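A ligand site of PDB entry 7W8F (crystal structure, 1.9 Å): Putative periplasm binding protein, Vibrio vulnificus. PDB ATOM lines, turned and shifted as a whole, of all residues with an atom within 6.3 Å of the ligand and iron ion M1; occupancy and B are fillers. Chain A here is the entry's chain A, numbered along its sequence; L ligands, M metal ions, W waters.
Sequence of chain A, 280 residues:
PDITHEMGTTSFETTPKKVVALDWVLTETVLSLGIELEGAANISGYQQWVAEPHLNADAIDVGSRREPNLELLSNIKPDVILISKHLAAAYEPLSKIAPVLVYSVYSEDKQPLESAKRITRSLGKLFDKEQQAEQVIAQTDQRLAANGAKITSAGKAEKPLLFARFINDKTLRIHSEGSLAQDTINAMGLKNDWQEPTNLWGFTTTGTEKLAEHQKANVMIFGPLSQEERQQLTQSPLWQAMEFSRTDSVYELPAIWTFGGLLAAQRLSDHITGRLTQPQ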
ATOM      1  N   TRP A  24      -0.008 -15.276  11.981  1.00  0.00           N
ATOM      2  CA  TRP A  24      -1.464 -15.214  12.229  1.00  0.00           C
ATOM      3  C   TRP A  24      -1.751 -15.045  13.708  1.00  0.00           C
ATOM      4  O   TRP A  24      -2.716 -14.373  14.009  1.00  0.00           O
ATOM      5  CB  TRP A  24      -2.109 -16.445  11.634  1.00  0.00           C
ATOM      6  CG  TRP A  24      -1.985 -16.494  10.150  1.00  0.00           C
ATOM      7  CD1 TRP A  24      -1.775 -15.443   9.306  1.00  0.00           C
ATOM      8  CD2 TRP A  24      -2.211 -17.640   9.318  1.00  0.00           C
ATOM      9  NE1 TRP A  24      -1.808 -15.875   8.008  1.00  0.00           N
ATOM     10  CE2 TRP A  24      -2.068 -17.212   7.983  1.00  0.00           C
ATOM     11  CE3 TRP A  24      -2.470 -18.982   9.574  1.00  0.00           C
ATOM     12  CZ2 TRP A  24      -2.212 -18.075   6.903  1.00  0.00           C
ATOM     13  CZ3 TRP A  24      -2.601 -19.840   8.499  1.00  0.00           C
ATOM     14  CH2 TRP A  24      -2.462 -19.385   7.187  1.00  0.00           C
ATOM     15  N   ASN A  42      -0.403 -13.429   4.274  1.00  0.00           N
ATOM     16  CA  ASN A  42      -1.344 -14.446   3.734  1.00  0.00           C
ATOM     17  C   ASN A  42      -2.732 -14.258   4.356  1.00  0.00           C
ATOM     18  O   ASN A  42      -3.125 -15.046   5.248  1.00  0.00           O
ATOM     19  CB  ASN A  42      -0.780 -15.863   3.881  1.00  0.00           C
ATOM     20  CG  ASN A  42      -1.628 -16.888   3.178  1.00  0.00           C
ATOM     21  OD1 ASN A  42      -2.607 -16.553   2.528  1.00  0.00           O
ATOM     22  ND2 ASN A  42      -1.265 -18.139   3.329  1.00  0.00           N
ATOM     23  N   GLY A  45      -5.221 -17.236   3.640  1.00  0.00           N
ATOM     24  CA  GLY A  45      -4.936 -18.275   4.668  1.00  0.00           C
ATOM     25  C   GLY A  45      -5.485 -17.901   6.043  1.00  0.00           C
ATOM     26  O   GLY A  45      -6.095 -18.775   6.692  1.00  0.00           O
ATOM     27  N   TRP A  49      -8.046 -20.480   7.777  1.00  0.00           N
ATOM     28  CA  TRP A  49      -7.554 -21.309   8.896  1.00  0.00           C
ATOM     29  C   TRP A  49      -7.816 -20.618  10.243  1.00  0.00           C
ATOM     30  O   TRP A  49      -7.855 -21.327  11.264  1.00  0.00           O
ATOM     31  CB  TRP A  49      -6.073 -21.651   8.689  1.00  0.00           C
ATOM     32  CG  TRP A  49      -5.821 -22.422   7.441  1.00  0.00           C
ATOM     33  CD1 TRP A  49      -5.340 -21.927   6.265  1.00  0.00           C
ATOM     34  CD2 TRP A  49      -6.017 -23.833   7.226  1.00  0.00           C
ATOM     35  NE1 TRP A  49      -5.237 -22.925   5.339  1.00  0.00           N
ATOM     36  CE2 TRP A  49      -5.646 -24.099   5.892  1.00  0.00           C
ATOM     37  CE3 TRP A  49      -6.471 -24.882   8.031  1.00  0.00           C
ATOM     38  CZ2 TRP A  49      -5.707 -25.382   5.339  1.00  0.00           C
ATOM     39  CZ3 TRP A  49      -6.543 -26.158   7.481  1.00  0.00           C
ATOM     40  CH2 TRP A  49      -6.162 -26.394   6.153  1.00  0.00           C
ATOM     41  N   ARG A  65       3.730 -16.070   5.050  1.00  0.00           N
ATOM     42  CA  ARG A  65       4.304 -16.047   6.410  1.00  0.00           C
ATOM     43  C   ARG A  65       5.823 -16.229   6.318  1.00  0.00           C
ATOM     44  O   ARG A  65       6.534 -15.648   7.157  1.00  0.00           O
ATOM     45  CB  ARG A  65       3.589 -17.113   7.259  1.00  0.00           C
ATOM     46  CG  ARG A  65       2.172 -16.715   7.637  1.00  0.00           C
ATOM     47  CD  ARG A  65       1.422 -17.776   8.428  1.00  0.00           C
ATOM     48  NE  ARG A  65       1.248 -18.954   7.578  1.00  0.00           N
ATOM     49  CZ  ARG A  65       1.079 -20.195   8.036  1.00  0.00           C
ATOM     50  NH1 ARG A  65       1.021 -20.442   9.335  1.00  0.00           N
ATOM     51  NH2 ARG A  65       0.964 -21.176   7.176  1.00  0.00           N
ATOM     52  N   ARG A 165      -5.743 -32.956  13.527  1.00  0.00           N
ATOM     53  CA  ARG A 165      -5.798 -32.233  12.244  1.00  0.00           C
ATOM     54  C   ARG A 165      -5.678 -33.289  11.131  1.00  0.00           C
ATOM     55  O   ARG A 165      -4.697 -34.022  11.105  1.00  0.00           O
ATOM     56  CB  ARG A 165      -4.668 -31.209  12.148  1.00  0.00           C
ATOM     57  CG  ARG A 165      -4.520 -30.554  10.785  1.00  0.00           C
ATOM     58  CD  ARG A 165      -5.580 -29.515  10.538  1.00  0.00           C
ATOM     59  NE  ARG A 165      -5.384 -28.307  11.329  1.00  0.00           N
ATOM     60  CZ  ARG A 165      -6.252 -27.304  11.360  1.00  0.00           C
ATOM     61  NH1 ARG A 165      -7.358 -27.375  10.644  1.00  0.00           N
ATOM     62  NH2 ARG A 165      -6.027 -26.222  12.095  1.00  0.00           N
ATOM     63  N   PHE A 166      -6.641 -33.343  10.222  1.00  0.00           N
ATOM     64  CA  PHE A 166      -6.525 -34.149   8.985  1.00  0.00           C
ATOM     65  C   PHE A 166      -5.432 -33.530   8.099  1.00  0.00           C
ATOM     66  O   PHE A 166      -5.576 -32.337   7.801  1.00  0.00           O
ATOM     67  CB  PHE A 166      -7.889 -34.171   8.302  1.00  0.00           C
ATOM     68  CG  PHE A 166      -7.974 -35.110   7.127  1.00  0.00           C
ATOM     69  CD1 PHE A 166      -7.426 -34.763   5.902  1.00  0.00           C
ATOM     70  CD2 PHE A 166      -8.628 -36.320   7.257  1.00  0.00           C
ATOM     71  CE1 PHE A 166      -7.528 -35.627   4.821  1.00  0.00           C
ATOM     72  CE2 PHE A 166      -8.733 -37.172   6.170  1.00  0.00           C
ATOM     73  CZ  PHE A 166      -8.177 -36.829   4.951  1.00  0.00           C
ATOM     74  N   ILE A 167      -4.392 -34.298   7.720  1.00  0.00           N
ATOM     75  CA  ILE A 167      -3.319 -33.894   6.762  1.00  0.00           C
ATOM     76  C   ILE A 167      -3.571 -34.572   5.416  1.00  0.00           C
ATOM     77  O   ILE A 167      -3.623 -33.854   4.414  1.00  0.00           O
ATOM     78  CB  ILE A 167      -1.893 -34.162   7.305  1.00  0.00           C
ATOM     79  CG1 ILE A 167      -1.682 -33.449   8.638  1.00  0.00           C
ATOM     80  CG2 ILE A 167      -0.814 -33.741   6.296  1.00  0.00           C
ATOM     81  CD1 ILE A 167      -1.870 -31.946   8.580  1.00  0.00           C
ATOM     82  N   ARG A 173      -2.083 -34.795  12.298  1.00  0.00           N
ATOM     83  CA  ARG A 173      -1.366 -34.140  13.414  1.00  0.00           C
ATOM     84  C   ARG A 173      -2.225 -34.314  14.665  1.00  0.00           C
ATOM     85  O   ARG A 173      -3.381 -33.877  14.640  1.00  0.00           O
ATOM     86  CB  ARG A 173      -1.151 -32.643  13.182  1.00  0.00           C
ATOM     87  CG  ARG A 173      -0.166 -32.301  12.080  1.00  0.00           C
ATOM     88  CD  ARG A 173      -0.163 -30.802  11.911  1.00  0.00           C
ATOM     89  NE  ARG A 173       0.761 -30.395  10.882  1.00  0.00           N
ATOM     90  CZ  ARG A 173       0.871 -29.154  10.428  1.00  0.00           C
ATOM     91  NH1 ARG A 173       0.131 -28.193  10.944  1.00  0.00           N
ATOM     92  NH2 ARG A 173       1.760 -28.871   9.500  1.00  0.00           N
ATOM     93  N   ASN A 199       6.357 -31.873  18.885  1.00  0.00           N
ATOM     94  CA  ASN A 199       7.345 -30.842  18.514  1.00  0.00           C
ATOM     95  C   ASN A 199       7.035 -29.577  19.342  1.00  0.00           C
ATOM     96  O   ASN A 199       6.070 -29.577  20.175  1.00  0.00           O
ATOM     97  CB  ASN A 199       7.343 -30.574  17.005  1.00  0.00           C
ATOM     98  CG  ASN A 199       5.963 -30.178  16.509  1.00  0.00           C
ATOM     99  OD1 ASN A 199       5.156 -29.649  17.257  1.00  0.00           O
ATOM    100  ND2 ASN A 199       5.687 -30.486  15.258  1.00  0.00           N
ATOM    101  N   TRP A 201       5.596 -27.011  18.426  1.00  0.00           N
ATOM    102  CA  TRP A 201       4.234 -26.507  18.127  1.00  0.00           C
ATOM    103  C   TRP A 201       3.137 -27.310  18.855  1.00  0.00           C
ATOM    104  O   TRP A 201       1.975 -26.972  18.696  1.00  0.00           O
ATOM    105  CB  TRP A 201       3.988 -26.445  16.613  1.00  0.00           C
ATOM    106  CG  TRP A 201       4.622 -25.220  16.019  1.00  0.00           C
ATOM    107  CD1 TRP A 201       4.113 -23.953  16.034  1.00  0.00           C
ATOM    108  CD2 TRP A 201       5.880 -25.136  15.363  1.00  0.00           C
ATOM    109  NE1 TRP A 201       4.969 -23.083  15.401  1.00  0.00           N
ATOM    110  CE2 TRP A 201       6.061 -23.780  14.986  1.00  0.00           C
ATOM    111  CE3 TRP A 201       6.861 -26.064  15.038  1.00  0.00           C
ATOM    112  CZ2 TRP A 201       7.193 -23.331  14.322  1.00  0.00           C
ATOM    113  CZ3 TRP A 201       7.988 -25.624  14.375  1.00  0.00           C
ATOM    114  CH2 TRP A 201       8.138 -24.283  14.011  1.00  0.00           C
ATOM    115  N   PHE A 203       2.399 -30.852  18.532  1.00  0.00           N
ATOM    116  CA  PHE A 203       1.727 -31.949  17.797  1.00  0.00           C
ATOM    117  C   PHE A 203       2.764 -32.986  17.378  1.00  0.00           C
ATOM    118  O   PHE A 203       3.972 -32.714  17.332  1.00  0.00           O
ATOM    119  CB  PHE A 203       0.917 -31.498  16.579  1.00  0.00           C
ATOM    120  CG  PHE A 203       1.696 -30.885  15.436  1.00  0.00           C
ATOM    121  CD1 PHE A 203       2.281 -31.695  14.460  1.00  0.00           C
ATOM    122  CD2 PHE A 203       1.818 -29.512  15.311  1.00  0.00           C
ATOM    123  CE1 PHE A 203       2.953 -31.131  13.387  1.00  0.00           C
ATOM    124  CE2 PHE A 203       2.509 -28.947  14.248  1.00  0.00           C
ATOM    125  CZ  PHE A 203       3.088 -29.751  13.302  1.00  0.00           C
ATOM    126  N   GLU A 229     -11.826 -33.882   1.806  1.00  0.00           N
ATOM    127  CA  GLU A 229     -11.326 -34.305   3.144  1.00  0.00           C
ATOM    128  C   GLU A 229     -12.471 -34.982   3.916  1.00  0.00           C
ATOM    129  O   GLU A 229     -12.258 -36.111   4.384  1.00  0.00           O
ATOM    130  CB  GLU A 229     -10.748 -33.114   3.923  1.00  0.00           C
ATOM    131  CG  GLU A 229      -9.393 -32.647   3.410  1.00  0.00           C
ATOM    132  CD  GLU A 229      -8.826 -31.378   4.043  1.00  0.00           C
ATOM    133  OE1 GLU A 229      -9.604 -30.534   4.561  1.00  0.00           O
ATOM    134  OE2 GLU A 229      -7.595 -31.236   4.001  1.00  0.00           O
ATOM    135  N   TRP A 257      -7.851 -21.676  14.790  1.00  0.00           N
ATOM    136  CA  TRP A 257      -6.423 -21.879  14.462  1.00  0.00           C
ATOM    137  C   TRP A 257      -5.745 -22.654  15.590  1.00  0.00           C
ATOM    138  O   TRP A 257      -5.805 -22.246  16.761  1.00  0.00           O
ATOM    139  CB  TRP A 257      -5.758 -20.531  14.235  1.00  0.00           C
ATOM    140  CG  TRP A 257      -4.370 -20.621  13.682  1.00  0.00           C
ATOM    141  CD1 TRP A 257      -3.359 -19.755  13.970  1.00  0.00           C
ATOM    142  CD2 TRP A 257      -3.844 -21.558  12.712  1.00  0.00           C
ATOM    143  NE1 TRP A 257      -2.255 -20.075  13.232  1.00  0.00           N
ATOM    144  CE2 TRP A 257      -2.509 -21.165  12.459  1.00  0.00           C
ATOM    145  CE3 TRP A 257      -4.374 -22.655  12.007  1.00  0.00           C
ATOM    146  CZ2 TRP A 257      -1.697 -21.836  11.553  1.00  0.00           C
ATOM    147  CZ3 TRP A 257      -3.564 -23.323  11.123  1.00  0.00           C
ATOM    148  CH2 TRP A 257      -2.235 -22.925  10.901  1.00  0.00           C
ATOM    149  N   THR A 258      -5.158 -23.793  15.240  1.00  0.00           N
ATOM    150  CA  THR A 258      -4.393 -24.669  16.167  1.00  0.00           C
ATOM    151  C   THR A 258      -3.110 -23.973  16.660  1.00  0.00           C
ATOM    152  O   THR A 258      -2.542 -24.472  17.643  1.00  0.00           O
ATOM    153  CB  THR A 258      -4.077 -25.998  15.465  1.00  0.00           C
ATOM    154  OG1 THR A 258      -3.644 -25.788  14.133  1.00  0.00           O
ATOM    155  CG2 THR A 258      -5.300 -26.887  15.383  1.00  0.00           C
ATOM    156  N   PHE A 259      -2.627 -22.933  15.971  1.00  0.00           N
ATOM    157  CA  PHE A 259      -1.419 -22.151  16.389  1.00  0.00           C
ATOM    158  C   PHE A 259      -1.816 -20.709  16.687  1.00  0.00           C
ATOM    159  O   PHE A 259      -1.043 -19.767  16.391  1.00  0.00           O
ATOM    160  CB  PHE A 259      -0.309 -22.309  15.347  1.00  0.00           C
ATOM    161  CG  PHE A 259      -0.100 -23.758  15.022  1.00  0.00           C
ATOM    162  CD1 PHE A 259       0.366 -24.617  15.993  1.00  0.00           C
ATOM    163  CD2 PHE A 259      -0.569 -24.285  13.834  1.00  0.00           C
ATOM    164  CE1 PHE A 259       0.485 -25.974  15.726  1.00  0.00           C
ATOM    165  CE2 PHE A 259      -0.465 -25.634  13.555  1.00  0.00           C
ATOM    166  CZ  PHE A 259       0.057 -26.480  14.517  1.00  0.00           C
HETATM  167  C1  LIG L   1       4.175 -26.182  12.454  1.00  0.00           C
HETATM  168  C2  LIG L   1       0.833 -26.809   4.715  1.00  0.00           C
HETATM  169  C3  LIG L   1       5.262 -25.617  11.573  1.00  0.00           C
HETATM  170  C4  LIG L   1       6.180 -26.699  11.009  1.00  0.00           C
HETATM  171  C5  LIG L   1       3.733 -25.098   7.404  1.00  0.00           C
HETATM  172  C6  LIG L   1       7.240 -26.159  10.038  1.00  0.00           C
HETATM  173  C7  LIG L   1       6.479 -25.027   7.998  1.00  0.00           C
HETATM  174  C8  LIG L   1       6.009 -25.071   6.559  1.00  0.00           C
HETATM  175  C9  LIG L   1       4.624 -24.502   6.318  1.00  0.00           C
HETATM  176  C10 LIG L   1       3.076 -27.131   5.887  1.00  0.00           C
HETATM  177  C11 LIG L   1       2.271 -26.357   4.835  1.00  0.00           C
HETATM  178  N1  LIG L   1       2.617 -24.643  11.492  1.00  0.00           N
HETATM  179  N2  LIG L   1       6.730 -26.154   8.631  1.00  0.00           N
HETATM  180  C12 LIG L   1       3.050 -25.204  12.787  1.00  0.00           C
HETATM  181  N3  LIG L   1       3.034 -26.389   7.179  1.00  0.00           N
HETATM  182  C13 LIG L   1       2.464 -22.251  12.298  1.00  0.00           C
HETATM  183  C14 LIG L   1       1.829 -23.462  11.581  1.00  0.00           C
HETATM  184  O1  LIG L   1       1.450 -23.143  10.278  1.00  0.00           O
HETATM  185  O2  LIG L   1       6.623 -23.968   8.553  1.00  0.00           O
HETATM  186  O3  LIG L   1       2.924 -24.082   7.958  1.00  0.00           O
HETATM  187  C15 LIG L   1       0.319 -26.332   3.360  1.00  0.00           C
HETATM  188  C16 LIG L   1       0.533 -24.848   3.084  1.00  0.00           C
HETATM  189  N4  LIG L   1      -0.176 -24.024   4.071  1.00  0.00           N
HETATM  190  C17 LIG L   1      -1.375 -24.160   4.648  1.00  0.00           C
HETATM  191  O4  LIG L   1      -2.135 -25.106   4.494  1.00  0.00           O
HETATM  192  C18 LIG L   1      -1.758 -23.074   5.626  1.00  0.00           C
HETATM  193  C19 LIG L   1      -2.204 -23.731   6.946  1.00  0.00           C
HETATM  194  C20 LIG L   1      -1.020 -24.540   7.533  1.00  0.00           C
HETATM  195  O5  LIG L   1       0.026 -23.670   7.850  1.00  0.00           O
HETATM  196  N5  LIG L   1      -1.291 -25.615   8.510  1.00  0.00           N
HETATM  197  C21 LIG L   1      -2.654 -25.895   8.968  1.00  0.00           C
HETATM  198  C22 LIG L   1      -3.244 -27.079   8.192  1.00  0.00           C
HETATM  199  C23 LIG L   1      -2.317 -28.194   7.719  1.00  0.00           C
HETATM  200  C24 LIG L   1      -2.555 -28.619   6.281  1.00  0.00           C
HETATM  201  O6  LIG L   1      -0.261 -25.790   9.547  1.00  0.00           O
HETATM  202  O7  LIG L   1       1.772 -26.451   7.945  1.00  0.00           O
HETATM  203  O8  LIG L   1       2.054 -25.726  10.715  1.00  0.00           O
HETATM  204 FE    FE M   1       1.325 -24.831   9.040  1.00  0.00          FE
HETATM  205 MG    MG M   2       0.746 -18.527  12.113  1.00  0.00          MG
HETATM  206 MG    MG M   3      -2.554 -28.396  12.987  1.00  0.00          MG
HETATM  207 FE    FE M   4       1.685 -18.677   4.409  1.00  0.00          FE
HETATM  208  O   HOH W   1       6.716 -28.750   8.151  1.00  0.00           O
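NE1 of Trp 49 touches C18 of the ligand (3.5 Å). Arg 165 touches the ligand. Ile 167 touches the ligand. Trp 201 touches the ligand. Phe 203 touches the ligand. Trp 257 touches the ligand (CZ3 to C21, 3.5 Å). CD2 of Phe 259 touches C14 of the ligand (3.4 Å). Hydrophobic or aromatic side chains within 4 Å of the ligand: Trp 49, Ile 167, Trp 201, Phe 203, Trp 257 and Phe 259. Of the 16 residues printed, 9 come within 4 Å of the ligand. The nearest printed residue that does not touch the ligand is Trp 24 (4.1 Å).
The guanidinium group (NH1) of Arg 173 sits close to an oxygen (O6) of the ligand (2.8 Å). The guanidinium group (NH2) of Arg 65 lies close to an oxygen (O5) of the ligand (2.7 Å).
No residue comes within 4 Å of iron ion M1.
Iron ion M1 is bound by O6 of the ligand. Iron ion M1 is bound by O7 of the ligand. Iron ion M1 is bound by O8 of the ligand, at 2.0 Å. O3 of the ligand is bound to iron ion M1, 2.1 Å away. An oxygen (O1) of the ligand binds iron ion M1. Iron ion M1 is bound by O5 of the ligand. Iron ion M1 has six donor atoms within binding distance.
The backbone NH (N) of Trp 201 is in hydrogen-bond range of the side-chain amide oxygen (OD1) of Asn 199, at 2.9 Å. O of Arg 173 lies within hydrogen-bond range of N of Arg 165. OD1 of Asn 199 is in hydrogen-bond range of N of Phe 203 (3.3 Å). NH2 of Arg 165 sits at hydrogen-bond distance from OG1 of Thr 258. The backbone carbonyl oxygen (O) of Phe 259 sits close to the indole nitrogen (NE1) of Trp 257 (3.4 Å).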
